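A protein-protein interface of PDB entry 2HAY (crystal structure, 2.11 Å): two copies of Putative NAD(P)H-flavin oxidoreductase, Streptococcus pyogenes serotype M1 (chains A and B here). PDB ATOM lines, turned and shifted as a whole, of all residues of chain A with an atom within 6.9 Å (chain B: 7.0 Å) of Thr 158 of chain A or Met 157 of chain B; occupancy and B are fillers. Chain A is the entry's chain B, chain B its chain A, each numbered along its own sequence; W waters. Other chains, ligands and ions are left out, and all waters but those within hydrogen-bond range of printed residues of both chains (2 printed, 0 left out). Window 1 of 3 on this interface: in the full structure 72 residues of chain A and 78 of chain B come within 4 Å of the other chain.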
ATOM      1  N   ILE A  12      39.374  14.775 -15.575  1.00  0.00           N
ATOM      2  CA  ILE A  12      38.609  13.526 -15.461  1.00  0.00           C
ATOM      3  C   ILE A  12      39.555  12.360 -15.212  1.00  0.00           C
ATOM      4  O   ILE A  12      39.316  11.547 -14.330  1.00  0.00           O
ATOM      5  CB  ILE A  12      37.757  13.238 -16.705  1.00  0.00           C
ATOM      6  CG1 ILE A  12      36.712  14.337 -16.891  1.00  0.00           C
ATOM      7  CG2 ILE A  12      37.038  11.852 -16.560  1.00  0.00           C
ATOM      8  CD1 ILE A  12      36.060  14.337 -18.268  1.00  0.00           C
ATOM      9  N   ASP A  34      30.701  21.560  -0.238  1.00  0.00           N
ATOM     10  CA  ASP A  34      31.082  20.332  -0.907  1.00  0.00           C
ATOM     11  C   ASP A  34      30.038  19.236  -0.698  1.00  0.00           C
ATOM     12  O   ASP A  34      29.705  18.556  -1.650  1.00  0.00           O
ATOM     13  CB  ASP A  34      32.465  19.862  -0.476  1.00  0.00           C
ATOM     14  CG  ASP A  34      33.600  20.715  -1.071  1.00  0.00           C
ATOM     15  OD1 ASP A  34      33.327  21.687  -1.803  1.00  0.00           O
ATOM     16  OD2 ASP A  34      34.779  20.413  -0.798  1.00  0.00           O
ATOM     17  N   LEU A  37      26.917  20.062  -2.923  1.00  0.00           N
ATOM     18  CA  LEU A  37      27.152  19.705  -4.321  1.00  0.00           C
ATOM     19  C   LEU A  37      27.060  18.205  -4.539  1.00  0.00           C
ATOM     20  O   LEU A  37      26.448  17.778  -5.513  1.00  0.00           O
ATOM     21  CB  LEU A  37      28.494  20.233  -4.818  1.00  0.00           C
ATOM     22  CG  LEU A  37      28.806  20.075  -6.309  1.00  0.00           C
ATOM     23  CD1 LEU A  37      27.742  20.735  -7.191  1.00  0.00           C
ATOM     24  CD2 LEU A  37      30.170  20.717  -6.565  1.00  0.00           C
ATOM     25  N   ILE A  38      27.631  17.419  -3.638  1.00  0.00           N
ATOM     26  CA  ILE A  38      27.568  15.967  -3.739  1.00  0.00           C
ATOM     27  C   ILE A  38      26.120  15.447  -3.683  1.00  0.00           C
ATOM     28  O   ILE A  38      25.731  14.559  -4.462  1.00  0.00           O
ATOM     29  CB  ILE A  38      28.446  15.269  -2.643  1.00  0.00           C
ATOM     30  CG1 ILE A  38      29.950  15.483  -2.916  1.00  0.00           C
ATOM     31  CG2 ILE A  38      28.126  13.744  -2.568  1.00  0.00           C
ATOM     32  CD1 ILE A  38      30.883  15.127  -1.694  1.00  0.00           C
ATOM     33  N   LEU A  39      25.324  16.029  -2.784  1.00  0.00           N
ATOM     34  CA  LEU A  39      23.934  15.660  -2.650  1.00  0.00           C
ATOM     35  C   LEU A  39      23.101  16.122  -3.855  1.00  0.00           C
ATOM     36  O   LEU A  39      22.167  15.439  -4.267  1.00  0.00           O
ATOM     37  CB  LEU A  39      23.367  16.199  -1.342  1.00  0.00           C
ATOM     38  CG  LEU A  39      23.789  15.450  -0.083  1.00  0.00           C
ATOM     39  CD1 LEU A  39      23.348  16.286   1.109  1.00  0.00           C
ATOM     40  CD2 LEU A  39      23.128  14.075  -0.052  1.00  0.00           C
ATOM     41  N   ASP A  40      23.445  17.284  -4.406  1.00  0.00           N
ATOM     42  CA  ASP A  40      22.846  17.783  -5.653  1.00  0.00           C
ATOM     43  C   ASP A  40      23.099  16.814  -6.807  1.00  0.00           C
ATOM     44  O   ASP A  40      22.228  16.639  -7.644  1.00  0.00           O
ATOM     45  CB  ASP A  40      23.414  19.138  -6.004  1.00  0.00           C
ATOM     46  CG  ASP A  40      22.602  20.290  -5.408  1.00  0.00           C
ATOM     47  OD1 ASP A  40      22.984  21.445  -5.661  1.00  0.00           O
ATOM     48  OD2 ASP A  40      21.590  20.059  -4.699  1.00  0.00           O
ATOM     49  N   ALA A  41      24.259  16.148  -6.801  1.00  0.00           N
ATOM     50  CA  ALA A  41      24.597  15.139  -7.810  1.00  0.00           C
ATOM     51  C   ALA A  41      23.651  13.931  -7.757  1.00  0.00           C
ATOM     52  O   ALA A  41      23.226  13.416  -8.794  1.00  0.00           O
ATOM     53  CB  ALA A  41      26.083  14.689  -7.672  1.00  0.00           C
ATOM     54  N   ALA A  42      23.315  13.491  -6.543  1.00  0.00           N
ATOM     55  CA  ALA A  42      22.328  12.417  -6.335  1.00  0.00           C
ATOM     56  C   ALA A  42      20.928  12.883  -6.736  1.00  0.00           C
ATOM     57  O   ALA A  42      20.216  12.229  -7.495  1.00  0.00           O
ATOM     58  CB  ALA A  42      22.357  11.979  -4.878  1.00  0.00           C
ATOM     59  N   GLY A 153      27.142   6.502  -8.087  1.00  0.00           N
ATOM     60  CA  GLY A 153      28.159   6.843  -9.055  1.00  0.00           C
ATOM     61  C   GLY A 153      28.379   8.344  -9.192  1.00  0.00           C
ATOM     62  O   GLY A 153      29.524   8.806  -9.182  1.00  0.00           O
ATOM     63  N   ASN A 154      27.286   9.098  -9.339  1.00  0.00           N
ATOM     64  CA  ASN A 154      27.406  10.543  -9.503  1.00  0.00           C
ATOM     65  C   ASN A 154      27.972  11.217  -8.272  1.00  0.00           C
ATOM     66  O   ASN A 154      28.773  12.129  -8.389  1.00  0.00           O
ATOM     67  CB  ASN A 154      26.072  11.177  -9.929  1.00  0.00           C
ATOM     68  CG  ASN A 154      25.742  10.879 -11.384  1.00  0.00           C
ATOM     69  OD1 ASN A 154      24.614  10.500 -11.731  1.00  0.00           O
ATOM     70  ND2 ASN A 154      26.739  11.022 -12.244  1.00  0.00           N
ATOM     71  N   MET A 155      27.553  10.766  -7.095  1.00  0.00           N
ATOM     72  CA  MET A 155      28.118  11.278  -5.843  1.00  0.00           C
ATOM     73  C   MET A 155      29.626  11.059  -5.733  1.00  0.00           C
ATOM     74  O   MET A 155      30.356  11.972  -5.383  1.00  0.00           O
ATOM     75  CB  MET A 155      27.398  10.675  -4.636  1.00  0.00           C
ATOM     76  CG  MET A 155      26.038  11.303  -4.436  1.00  0.00           C
ATOM     77  SD  MET A 155      25.308  10.924  -2.684  1.00  0.00           S
ATOM     78  CE  MET A 155      24.796   9.088  -2.941  1.00  0.00           C
ATOM     79  N   MET A 156      30.064   9.836  -6.014  1.00  0.00           N
ATOM     80  CA  MET A 156      31.468   9.455  -5.935  1.00  0.00           C
ATOM     81  C   MET A 156      32.361  10.169  -6.937  1.00  0.00           C
ATOM     82  O   MET A 156      33.493  10.481  -6.599  1.00  0.00           O
ATOM     83  CB  MET A 156      31.633   7.953  -6.101  1.00  0.00           C
ATOM     84  CG  MET A 156      31.132   7.152  -4.875  1.00  0.00           C
ATOM     85  SD  MET A 156      31.703   5.303  -5.033  1.00  0.00           S
ATOM     86  CE  MET A 156      30.599   4.837  -6.548  1.00  0.00           C
ATOM     87  N   MET A 157      31.860  10.410  -8.152  1.00  0.00           N
ATOM     88  CA  MET A 157      32.601  11.189  -9.158  1.00  0.00           C
ATOM     89  C   MET A 157      32.726  12.660  -8.756  1.00  0.00           C
ATOM     90  O   MET A 157      33.813  13.255  -8.853  1.00  0.00           O
ATOM     91  CB  MET A 157      31.971  11.071 -10.558  1.00  0.00           C
ATOM     92  CG  MET A 157      32.737  11.851 -11.641  1.00  0.00           C
ATOM     93  SD  MET A 157      34.601  11.269 -11.816  1.00  0.00           S
ATOM     94  CE  MET A 157      34.214   9.632 -12.788  1.00  0.00           C
ATOM     95  N   THR A 158      31.612  13.234  -8.316  1.00  0.00           N
ATOM     96  CA  THR A 158      31.589  14.584  -7.761  1.00  0.00           C
ATOM     97  C   THR A 158      32.567  14.705  -6.585  1.00  0.00           C
ATOM     98  O   THR A 158      33.405  15.576  -6.606  1.00  0.00           O
ATOM     99  CB  THR A 158      30.154  14.975  -7.350  1.00  0.00           C
ATOM    100  OG1 THR A 158      29.309  14.846  -8.498  1.00  0.00           O
ATOM    101  CG2 THR A 158      30.091  16.434  -6.839  1.00  0.00           C
ATOM    102  N   ALA A 159      32.490  13.800  -5.594  1.00  0.00           N
ATOM    103  CA  ALA A 159      33.493  13.742  -4.529  1.00  0.00           C
ATOM    104  C   ALA A 159      34.929  13.669  -5.065  1.00  0.00           C
ATOM    105  O   ALA A 159      35.785  14.399  -4.613  1.00  0.00           O
ATOM    106  CB  ALA A 159      33.210  12.565  -3.561  1.00  0.00           C
ATOM    107  N   ALA A 160      35.179  12.803  -6.046  1.00  0.00           N
ATOM    108  CA  ALA A 160      36.521  12.608  -6.567  1.00  0.00           C
ATOM    109  C   ALA A 160      37.086  13.895  -7.191  1.00  0.00           C
ATOM    110  O   ALA A 160      38.221  14.254  -6.924  1.00  0.00           O
ATOM    111  CB  ALA A 160      36.546  11.471  -7.570  1.00  0.00           C
ATOM    112  N   LEU A 161      36.261  14.585  -7.982  1.00  0.00           N
ATOM    113  CA  LEU A 161      36.599  15.869  -8.606  1.00  0.00           C
ATOM    114  C   LEU A 161      36.886  16.963  -7.570  1.00  0.00           C
ATOM    115  O   LEU A 161      37.639  17.908  -7.828  1.00  0.00           O
ATOM    116  CB  LEU A 161      35.478  16.312  -9.551  1.00  0.00           C
ATOM    117  CG  LEU A 161      35.368  15.525 -10.847  1.00  0.00           C
ATOM    118  CD1 LEU A 161      33.951  15.649 -11.446  1.00  0.00           C
ATOM    119  CD2 LEU A 161      36.427  15.922 -11.901  1.00  0.00           C
ATOM    120  N   LEU A 162      36.305  16.786  -6.391  1.00  0.00           N
ATOM    121  CA  LEU A 162      36.490  17.681  -5.279  1.00  0.00           C
ATOM    122  C   LEU A 162      37.682  17.279  -4.391  1.00  0.00           C
ATOM    123  O   LEU A 162      38.074  18.028  -3.504  1.00  0.00           O
ATOM    124  CB  LEU A 162      35.189  17.720  -4.470  1.00  0.00           C
ATOM    125  CG  LEU A 162      34.030  18.513  -5.097  1.00  0.00           C
ATOM    126  CD1 LEU A 162      32.817  18.404  -4.173  1.00  0.00           C
ATOM    127  CD2 LEU A 162      34.415  20.005  -5.344  1.00  0.00           C
ATOM    128  N   GLY A 163      38.270  16.115  -4.643  1.00  0.00           N
ATOM    129  CA  GLY A 163      39.352  15.602  -3.789  1.00  0.00           C
ATOM    130  C   GLY A 163      38.866  14.905  -2.540  1.00  0.00           C
ATOM    131  O   GLY A 163      39.636  14.649  -1.632  1.00  0.00           O
ATOM    132  N   ILE A 164      37.569  14.586  -2.505  1.00  0.00           N
ATOM    133  CA  ILE A 164      36.945  13.948  -1.364  1.00  0.00           C
ATOM    134  C   ILE A 164      36.963  12.440  -1.621  1.00  0.00           C
ATOM    135  O   ILE A 164      36.545  11.977  -2.681  1.00  0.00           O
ATOM    136  CB  ILE A 164      35.504  14.494  -1.145  1.00  0.00           C
ATOM    137  CG1 ILE A 164      35.571  15.966  -0.724  1.00  0.00           C
ATOM    138  CG2 ILE A 164      34.714  13.627  -0.144  1.00  0.00           C
ATOM    139  CD1 ILE A 164      34.219  16.668  -0.749  1.00  0.00           C
ATOM    140  N   ILE B   8      35.668  24.615  -9.638  1.00  0.00           N
ATOM    141  CA  ILE B   8      35.191  23.209  -9.864  1.00  0.00           C
ATOM    142  C   ILE B   8      33.699  23.057  -9.539  1.00  0.00           C
ATOM    143  O   ILE B   8      33.009  22.248 -10.158  1.00  0.00           O
ATOM    144  CB  ILE B   8      36.058  22.169  -9.086  1.00  0.00           C
ATOM    145  CG1 ILE B   8      37.523  22.261  -9.535  1.00  0.00           C
ATOM    146  CG2 ILE B   8      35.571  20.743  -9.343  1.00  0.00           C
ATOM    147  CD1 ILE B   8      38.569  21.857  -8.464  1.00  0.00           C
ATOM    148  N   GLN B  11      31.602  24.331 -12.513  1.00  0.00           N
ATOM    149  CA  GLN B  11      31.794  23.319 -13.552  1.00  0.00           C
ATOM    150  C   GLN B  11      30.949  22.060 -13.315  1.00  0.00           C
ATOM    151  O   GLN B  11      30.212  21.618 -14.214  1.00  0.00           O
ATOM    152  CB  GLN B  11      33.280  22.968 -13.628  1.00  0.00           C
ATOM    153  CG  GLN B  11      33.685  22.137 -14.832  1.00  0.00           C
ATOM    154  CD  GLN B  11      35.018  21.442 -14.614  1.00  0.00           C
ATOM    155  OE1 GLN B  11      35.674  21.635 -13.579  1.00  0.00           O
ATOM    156  NE2 GLN B  11      35.426  20.622 -15.587  1.00  0.00           N
ATOM    157  N   ILE B  12      31.034  21.491 -12.109  1.00  0.00           N
ATOM    158  CA  ILE B  12      30.202  20.337 -11.762  1.00  0.00           C
ATOM    159  C   ILE B  12      28.709  20.660 -11.924  1.00  0.00           C
ATOM    160  O   ILE B  12      27.965  19.919 -12.582  1.00  0.00           O
ATOM    161  CB  ILE B  12      30.539  19.740 -10.354  1.00  0.00           C
ATOM    162  CG1 ILE B  12      31.983  19.245 -10.323  1.00  0.00           C
ATOM    163  CG2 ILE B  12      29.600  18.556 -10.008  1.00  0.00           C
ATOM    164  CD1 ILE B  12      32.465  18.815  -8.945  1.00  0.00           C
ATOM    165  N   ALA B  15      27.681  20.670 -15.413  1.00  0.00           N
ATOM    166  CA  ALA B  15      27.520  19.312 -15.933  1.00  0.00           C
ATOM    167  C   ALA B  15      26.208  18.663 -15.479  1.00  0.00           C
ATOM    168  O   ALA B  15      25.603  17.907 -16.223  1.00  0.00           O
ATOM    169  CB  ALA B  15      28.719  18.424 -15.557  1.00  0.00           C
ATOM    170  N   LEU B  16      25.783  18.957 -14.249  1.00  0.00           N
ATOM    171  CA  LEU B  16      24.572  18.353 -13.666  1.00  0.00           C
ATOM    172  C   LEU B  16      23.323  18.851 -14.367  1.00  0.00           C
ATOM    173  O   LEU B  16      22.368  18.096 -14.572  1.00  0.00           O
ATOM    174  CB  LEU B  16      24.493  18.614 -12.149  1.00  0.00           C
ATOM    175  CG  LEU B  16      25.545  17.876 -11.314  1.00  0.00           C
ATOM    176  CD1 LEU B  16      25.631  18.388  -9.879  1.00  0.00           C
ATOM    177  CD2 LEU B  16      25.281  16.365 -11.371  1.00  0.00           C
ATOM    178  N   ARG B  19      23.411  17.521 -18.327  1.00  0.00           N
ATOM    179  CA  ARG B  19      22.964  16.154 -18.611  1.00  0.00           C
ATOM    180  C   ARG B  19      21.429  16.084 -18.606  1.00  0.00           C
ATOM    181  O   ARG B  19      20.798  16.394 -17.601  1.00  0.00           O
ATOM    182  CB  ARG B  19      23.529  15.104 -17.636  1.00  0.00           C
ATOM    183  CG  ARG B  19      23.337  13.686 -18.171  1.00  0.00           C
ATOM    184  CD  ARG B  19      23.009  12.654 -17.098  1.00  0.00           C
ATOM    185  NE  ARG B  19      21.974  13.194 -16.230  1.00  0.00           N
ATOM    186  CZ  ARG B  19      20.666  13.206 -16.476  1.00  0.00           C
ATOM    187  NH1 ARG B  19      20.157  12.647 -17.566  1.00  0.00           N
ATOM    188  NH2 ARG B  19      19.862  13.765 -15.586  1.00  0.00           N
ATOM    189  N   ALA B 151      28.627   2.328 -13.030  1.00  0.00           N
ATOM    190  CA  ALA B 151      29.369   2.612 -14.280  1.00  0.00           C
ATOM    191  C   ALA B 151      28.517   3.456 -15.208  1.00  0.00           C
ATOM    192  O   ALA B 151      29.010   4.360 -15.888  1.00  0.00           O
ATOM    193  CB  ALA B 151      29.721   1.296 -14.967  1.00  0.00           C
ATOM    194  N   LEU B 152      27.224   3.161 -15.239  1.00  0.00           N
ATOM    195  CA  LEU B 152      26.302   3.959 -16.005  1.00  0.00           C
ATOM    196  C   LEU B 152      26.329   5.443 -15.583  1.00  0.00           C
ATOM    197  O   LEU B 152      26.424   6.316 -16.436  1.00  0.00           O
ATOM    198  CB  LEU B 152      24.907   3.399 -15.861  1.00  0.00           C
ATOM    199  CG  LEU B 152      23.809   4.109 -16.653  1.00  0.00           C
ATOM    200  CD1 LEU B 152      24.007   3.906 -18.168  1.00  0.00           C
ATOM    201  CD2 LEU B 152      22.466   3.565 -16.191  1.00  0.00           C
ATOM    202  N   GLY B 153      26.284   5.716 -14.274  1.00  0.00           N
ATOM    203  CA  GLY B 153      26.378   7.095 -13.744  1.00  0.00           C
ATOM    204  C   GLY B 153      27.742   7.729 -14.018  1.00  0.00           C
ATOM    205  O   GLY B 153      27.815   8.887 -14.449  1.00  0.00           O
ATOM    206  N   ASN B 154      28.822   6.984 -13.781  1.00  0.00           N
ATOM    207  CA  ASN B 154      30.189   7.442 -14.136  1.00  0.00           C
ATOM    208  C   ASN B 154      30.379   7.796 -15.636  1.00  0.00           C
ATOM    209  O   ASN B 154      31.010   8.780 -15.953  1.00  0.00           O
ATOM    210  CB  ASN B 154      31.244   6.416 -13.690  1.00  0.00           C
ATOM    211  CG  ASN B 154      31.375   6.335 -12.173  1.00  0.00           C
ATOM    212  OD1 ASN B 154      31.064   7.296 -11.470  1.00  0.00           O
ATOM    213  ND2 ASN B 154      31.863   5.209 -11.665  1.00  0.00           N
ATOM    214  N   MET B 155      29.816   6.997 -16.541  1.00  0.00           N
ATOM    215  CA  MET B 155      29.906   7.279 -17.979  1.00  0.00           C
ATOM    216  C   MET B 155      29.150   8.550 -18.325  1.00  0.00           C
ATOM    217  O   MET B 155      29.652   9.352 -19.085  1.00  0.00           O
ATOM    218  CB  MET B 155      29.392   6.112 -18.826  1.00  0.00           C
ATOM    219  CG  MET B 155      30.406   4.998 -18.959  1.00  0.00           C
ATOM    220  SD  MET B 155      29.892   3.624 -20.228  1.00  0.00           S
ATOM    221  CE  MET B 155      28.446   2.737 -19.297  1.00  0.00           C
ATOM    222  N   MET B 156      27.951   8.711 -17.762  1.00  0.00           N
ATOM    223  CA  MET B 156      27.110   9.888 -18.025  1.00  0.00           C
ATOM    224  C   MET B 156      27.692  11.173 -17.516  1.00  0.00           C
ATOM    225  O   MET B 156      27.605  12.194 -18.190  1.00  0.00           O
ATOM    226  CB  MET B 156      25.688   9.709 -17.509  1.00  0.00           C
ATOM    227  CG  MET B 156      24.879   8.669 -18.308  1.00  0.00           C
ATOM    228  SD  MET B 156      23.016   8.617 -17.763  1.00  0.00           S
ATOM    229  CE  MET B 156      23.248   7.922 -15.952  1.00  0.00           C
ATOM    230  N   MET B 157      28.288  11.132 -16.329  1.00  0.00           N
ATOM    231  CA  MET B 157      28.952  12.297 -15.761  1.00  0.00           C
ATOM    232  C   MET B 157      30.200  12.705 -16.570  1.00  0.00           C
ATOM    233  O   MET B 157      30.413  13.891 -16.808  1.00  0.00           O
ATOM    234  CB  MET B 157      29.357  12.065 -14.302  1.00  0.00           C
ATOM    235  CG  MET B 157      30.215  13.223 -13.756  1.00  0.00           C
ATOM    236  SD  MET B 157      29.093  14.818 -13.494  1.00  0.00           S
ATOM    237  CE  MET B 157      28.420  14.151 -11.793  1.00  0.00           C
ATOM    238  N   THR B 158      31.027  11.719 -16.922  1.00  0.00           N
ATOM    239  CA  THR B 158      32.190  11.927 -17.789  1.00  0.00           C
ATOM    240  C   THR B 158      31.737  12.564 -19.121  1.00  0.00           C
ATOM    241  O   THR B 158      32.267  13.587 -19.521  1.00  0.00           O
ATOM    242  CB  THR B 158      32.912  10.593 -18.033  1.00  0.00           C
ATOM    243  OG1 THR B 158      33.313  10.048 -16.766  1.00  0.00           O
ATOM    244  CG2 THR B 158      34.167  10.780 -18.925  1.00  0.00           C
ATOM    245  N   ALA B 159      30.751  11.938 -19.773  1.00  0.00           N
ATOM    246  CA  ALA B 159      30.138  12.456 -20.989  1.00  0.00           C
ATOM    247  C   ALA B 159      29.753  13.925 -20.811  1.00  0.00           C
ATOM    248  O   ALA B 159      30.214  14.762 -21.566  1.00  0.00           O
ATOM    249  CB  ALA B 159      28.930  11.612 -21.361  1.00  0.00           C
ATOM    250  N   ALA B 160      28.948  14.230 -19.794  1.00  0.00           N
ATOM    251  CA  ALA B 160      28.467  15.592 -19.535  1.00  0.00           C
ATOM    252  C   ALA B 160      29.597  16.586 -19.353  1.00  0.00           C
ATOM    253  O   ALA B 160      29.533  17.695 -19.886  1.00  0.00           O
ATOM    254  CB  ALA B 160      27.560  15.612 -18.334  1.00  0.00           C
ATOM    255  N   LEU B 161      30.613  16.209 -18.582  1.00  0.00           N
ATOM    256  CA  LEU B 161      31.813  17.042 -18.414  1.00  0.00           C
ATOM    257  C   LEU B 161      32.555  17.297 -19.738  1.00  0.00           C
ATOM    258  O   LEU B 161      33.242  18.297 -19.877  1.00  0.00           O
ATOM    259  CB  LEU B 161      32.737  16.424 -17.378  1.00  0.00           C
ATOM    260  CG  LEU B 161      32.318  16.485 -15.877  1.00  0.00           C
ATOM    261  CD1 LEU B 161      33.141  15.483 -15.101  1.00  0.00           C
ATOM    262  CD2 LEU B 161      32.489  17.903 -15.265  1.00  0.00           C
ATOM    263  N   LEU B 162      32.400  16.398 -20.707  1.00  0.00           N
ATOM    264  CA  LEU B 162      32.921  16.617 -22.045  1.00  0.00           C
ATOM    265  C   LEU B 162      31.927  17.312 -22.991  1.00  0.00           C
ATOM    266  O   LEU B 162      32.257  17.571 -24.157  1.00  0.00           O
ATOM    267  CB  LEU B 162      33.345  15.299 -22.660  1.00  0.00           C
ATOM    268  CG  LEU B 162      34.417  14.539 -21.872  1.00  0.00           C
ATOM    269  CD1 LEU B 162      34.312  13.080 -22.257  1.00  0.00           C
ATOM    270  CD2 LEU B 162      35.809  15.150 -22.186  1.00  0.00           C
ATOM    271  N   GLY B 163      30.733  17.643 -22.504  1.00  0.00           N
ATOM    272  CA  GLY B 163      29.739  18.277 -23.382  1.00  0.00           C
ATOM    273  C   GLY B 163      29.090  17.248 -24.304  1.00  0.00           C
ATOM    274  O   GLY B 163      28.541  17.595 -25.338  1.00  0.00           O
ATOM    275  N   ILE B 164      29.125  15.984 -23.910  1.00  0.00           N
ATOM    276  CA  ILE B 164      28.505  14.927 -24.697  1.00  0.00           C
ATOM    277  C   ILE B 164      27.215  14.487 -24.069  1.00  0.00           C
ATOM    278  O   ILE B 164      27.151  14.265 -22.875  1.00  0.00           O
ATOM    279  CB  ILE B 164      29.436  13.720 -24.864  1.00  0.00           C
ATOM    280  CG1 ILE B 164      30.603  14.120 -25.768  1.00  0.00           C
ATOM    281  CG2 ILE B 164      28.663  12.517 -25.443  1.00  0.00           C
ATOM    282  CD1 ILE B 164      31.806  13.195 -25.707  1.00  0.00           C
ATOM    283  N   THR B 166      23.770  12.031 -23.447  1.00  0.00           N
ATOM    284  CA  THR B 166      23.538  10.619 -23.249  1.00  0.00           C
ATOM    285  C   THR B 166      22.054  10.370 -22.985  1.00  0.00           C
ATOM    286  O   THR B 166      21.279  11.299 -22.810  1.00  0.00           O
ATOM    287  CB  THR B 166      24.380  10.055 -22.050  1.00  0.00           C
ATOM    288  OG1 THR B 166      24.026  10.720 -20.826  1.00  0.00           O
ATOM    289  CG2 THR B 166      25.869  10.208 -22.299  1.00  0.00           C
HETATM  290  O   HOH W   1      24.823  10.476 -14.340  1.00  0.00           O
HETATM  291  O   HOH W   2      32.150   6.956  -9.255  1.00  0.00           O
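O of Asn 154 of chain A is in hydrogen-bond range of OG1 of Thr 158 of chain A (2.8 Å).
OG1 of Thr 158 of chain B is in hydrogen-bond range of O of Asn 154 of chain B (2.8 Å).
Asp 34 of chain A touches none of the printed residues of chain B.
Printed residues of chain B within 4 Å of Leu 37 of chain A: Ile 12 (3.8 Å).
Thr 158 of chain A touches just these residues of chain B: Ile 12 (3.8 Å) and Met 157 (3.5 Å).
Of the printed residues of chain A, Ile 8 of chain B touches Leu 161.
Of the printed residues of chain A, Ile 12 of chain B touches Leu 37 (3.8 Å), Thr 158 (3.8 Å) and Leu 161 (3.96 Å).
Of the printed residues of chain A, Gly 153 of chain B touches Asn 154 (3.3 Å).
Of the printed residues of chain A, Asn 154 of chain B touches Gly 153 (3.1 Å) and Met 157 (3.99 Å).
Met 156 of chain B touches none of the printed residues of chain A.
Of the printed residues of chain A, Met 157 of chain B touches Asn 154 (3.5 Å), Met 157 (3.6 Å) and Thr 158 (3.5 Å).
The nearest residue of chain B that does not touch Thr 158 of chain A is Leu 16 of chain B (5.2 Å).
The nearest printed residue of chain A that does not touch Met 157 of chain B is Ala 41 of chain A (4.8 Å).
Water W2 lies within hydrogen-bond range of OD1 of Asn 154 of chain B and O of Gly 153 of chain A.
Water W1 bridges the side-chain amide oxygen of Asn 154 of chain A and the backbone carbonyl oxygen of Gly 153 of chain B.
The side-chain amide oxygen (OD1) of Asn 154 of chain B sits close to the backbone carbonyl oxygen (O) of Gly 153 of chain A.
O of Gly 153 of chain B sits at hydrogen-bond distance from ND2 of Asn 154 of chain A, at 3.3 Å.
Gly 153 of chain A touches Asn 154 of chain B, and with the chains exchanged Asn 154 of chain A touches Gly 153 of chain B.
Met 157 of chain B touches its own counterpart, Met 157 of chain A.
Leu 161 of chain A touches Ile 12 of chain B, but with the chains exchanged Ile 12 of chain A does not touch Leu 161 of chain B (4.02 Å).
Leu 161 of chain B touches its own counterpart, Leu 161 of chain A.
Of the 14 pairs that touch across the chains among the printed residues, 8 have their exchanged pair printed and touching as well.
Of the 21 printed residues of chain B, 9 touch a printed residue of chain A.
Printed residues of chain B that touch a printed residue of chain A: Ile 8, Ile 12, Leu 16, Gly 153, Asn 154, Met 157, Thr 158, Leu 161 and Leu 162.
Hydrophobic or aromatic side chains of chain B within 4 Å of the printed part of chain A: Ile 8, Ile 12, Leu 16, Met 157, Leu 161 and Leu 162.
Of the 20 printed residues of chain A, 8 touch a printed residue of chain B.
Hydrophobic or aromatic side chains of chain A that line the printed part of chain B: Ile 12, Leu 37, Met 157 and Leu 161.
Among the printed residues, 14 pairs touch across the chains.
Among the printed residues, no Asp or Glu carboxylate lies within 4 Å of a Lys or Arg side-chain nitrogen of the other chain.
Among the printed residues, pairs that only touch across the chains: Ile 12 of chain A with Thr 158 of chain B (3.9 Å), Ile 12 of chain A with Leu 162 of chain B (3.97 Å), Leu 37 of chain A with Ile 12 of chain B (3.8 Å), Ala 41 of chain A with Leu 16 of chain B (3.8 Å), Asn 154 of chain A with Met 157 of chain B (3.5 Å), Met 157 of chain A with Asn 154 of chain B (3.99 Å), Met 157 of chain A with Met 157 of chain B (3.6 Å), Thr 158 of chain A with Ile 12 of chain B (3.8 Å), Thr 158 of chain A with Met 157 of chain B (3.5 Å), Leu 161 of chain A with Ile 8 of chain B (3.8 Å), Leu 161 of chain A with Ile 12 of chain B (3.96 Å) and Leu 161 of chain A with Leu 161 of chain B (3.7 Å).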
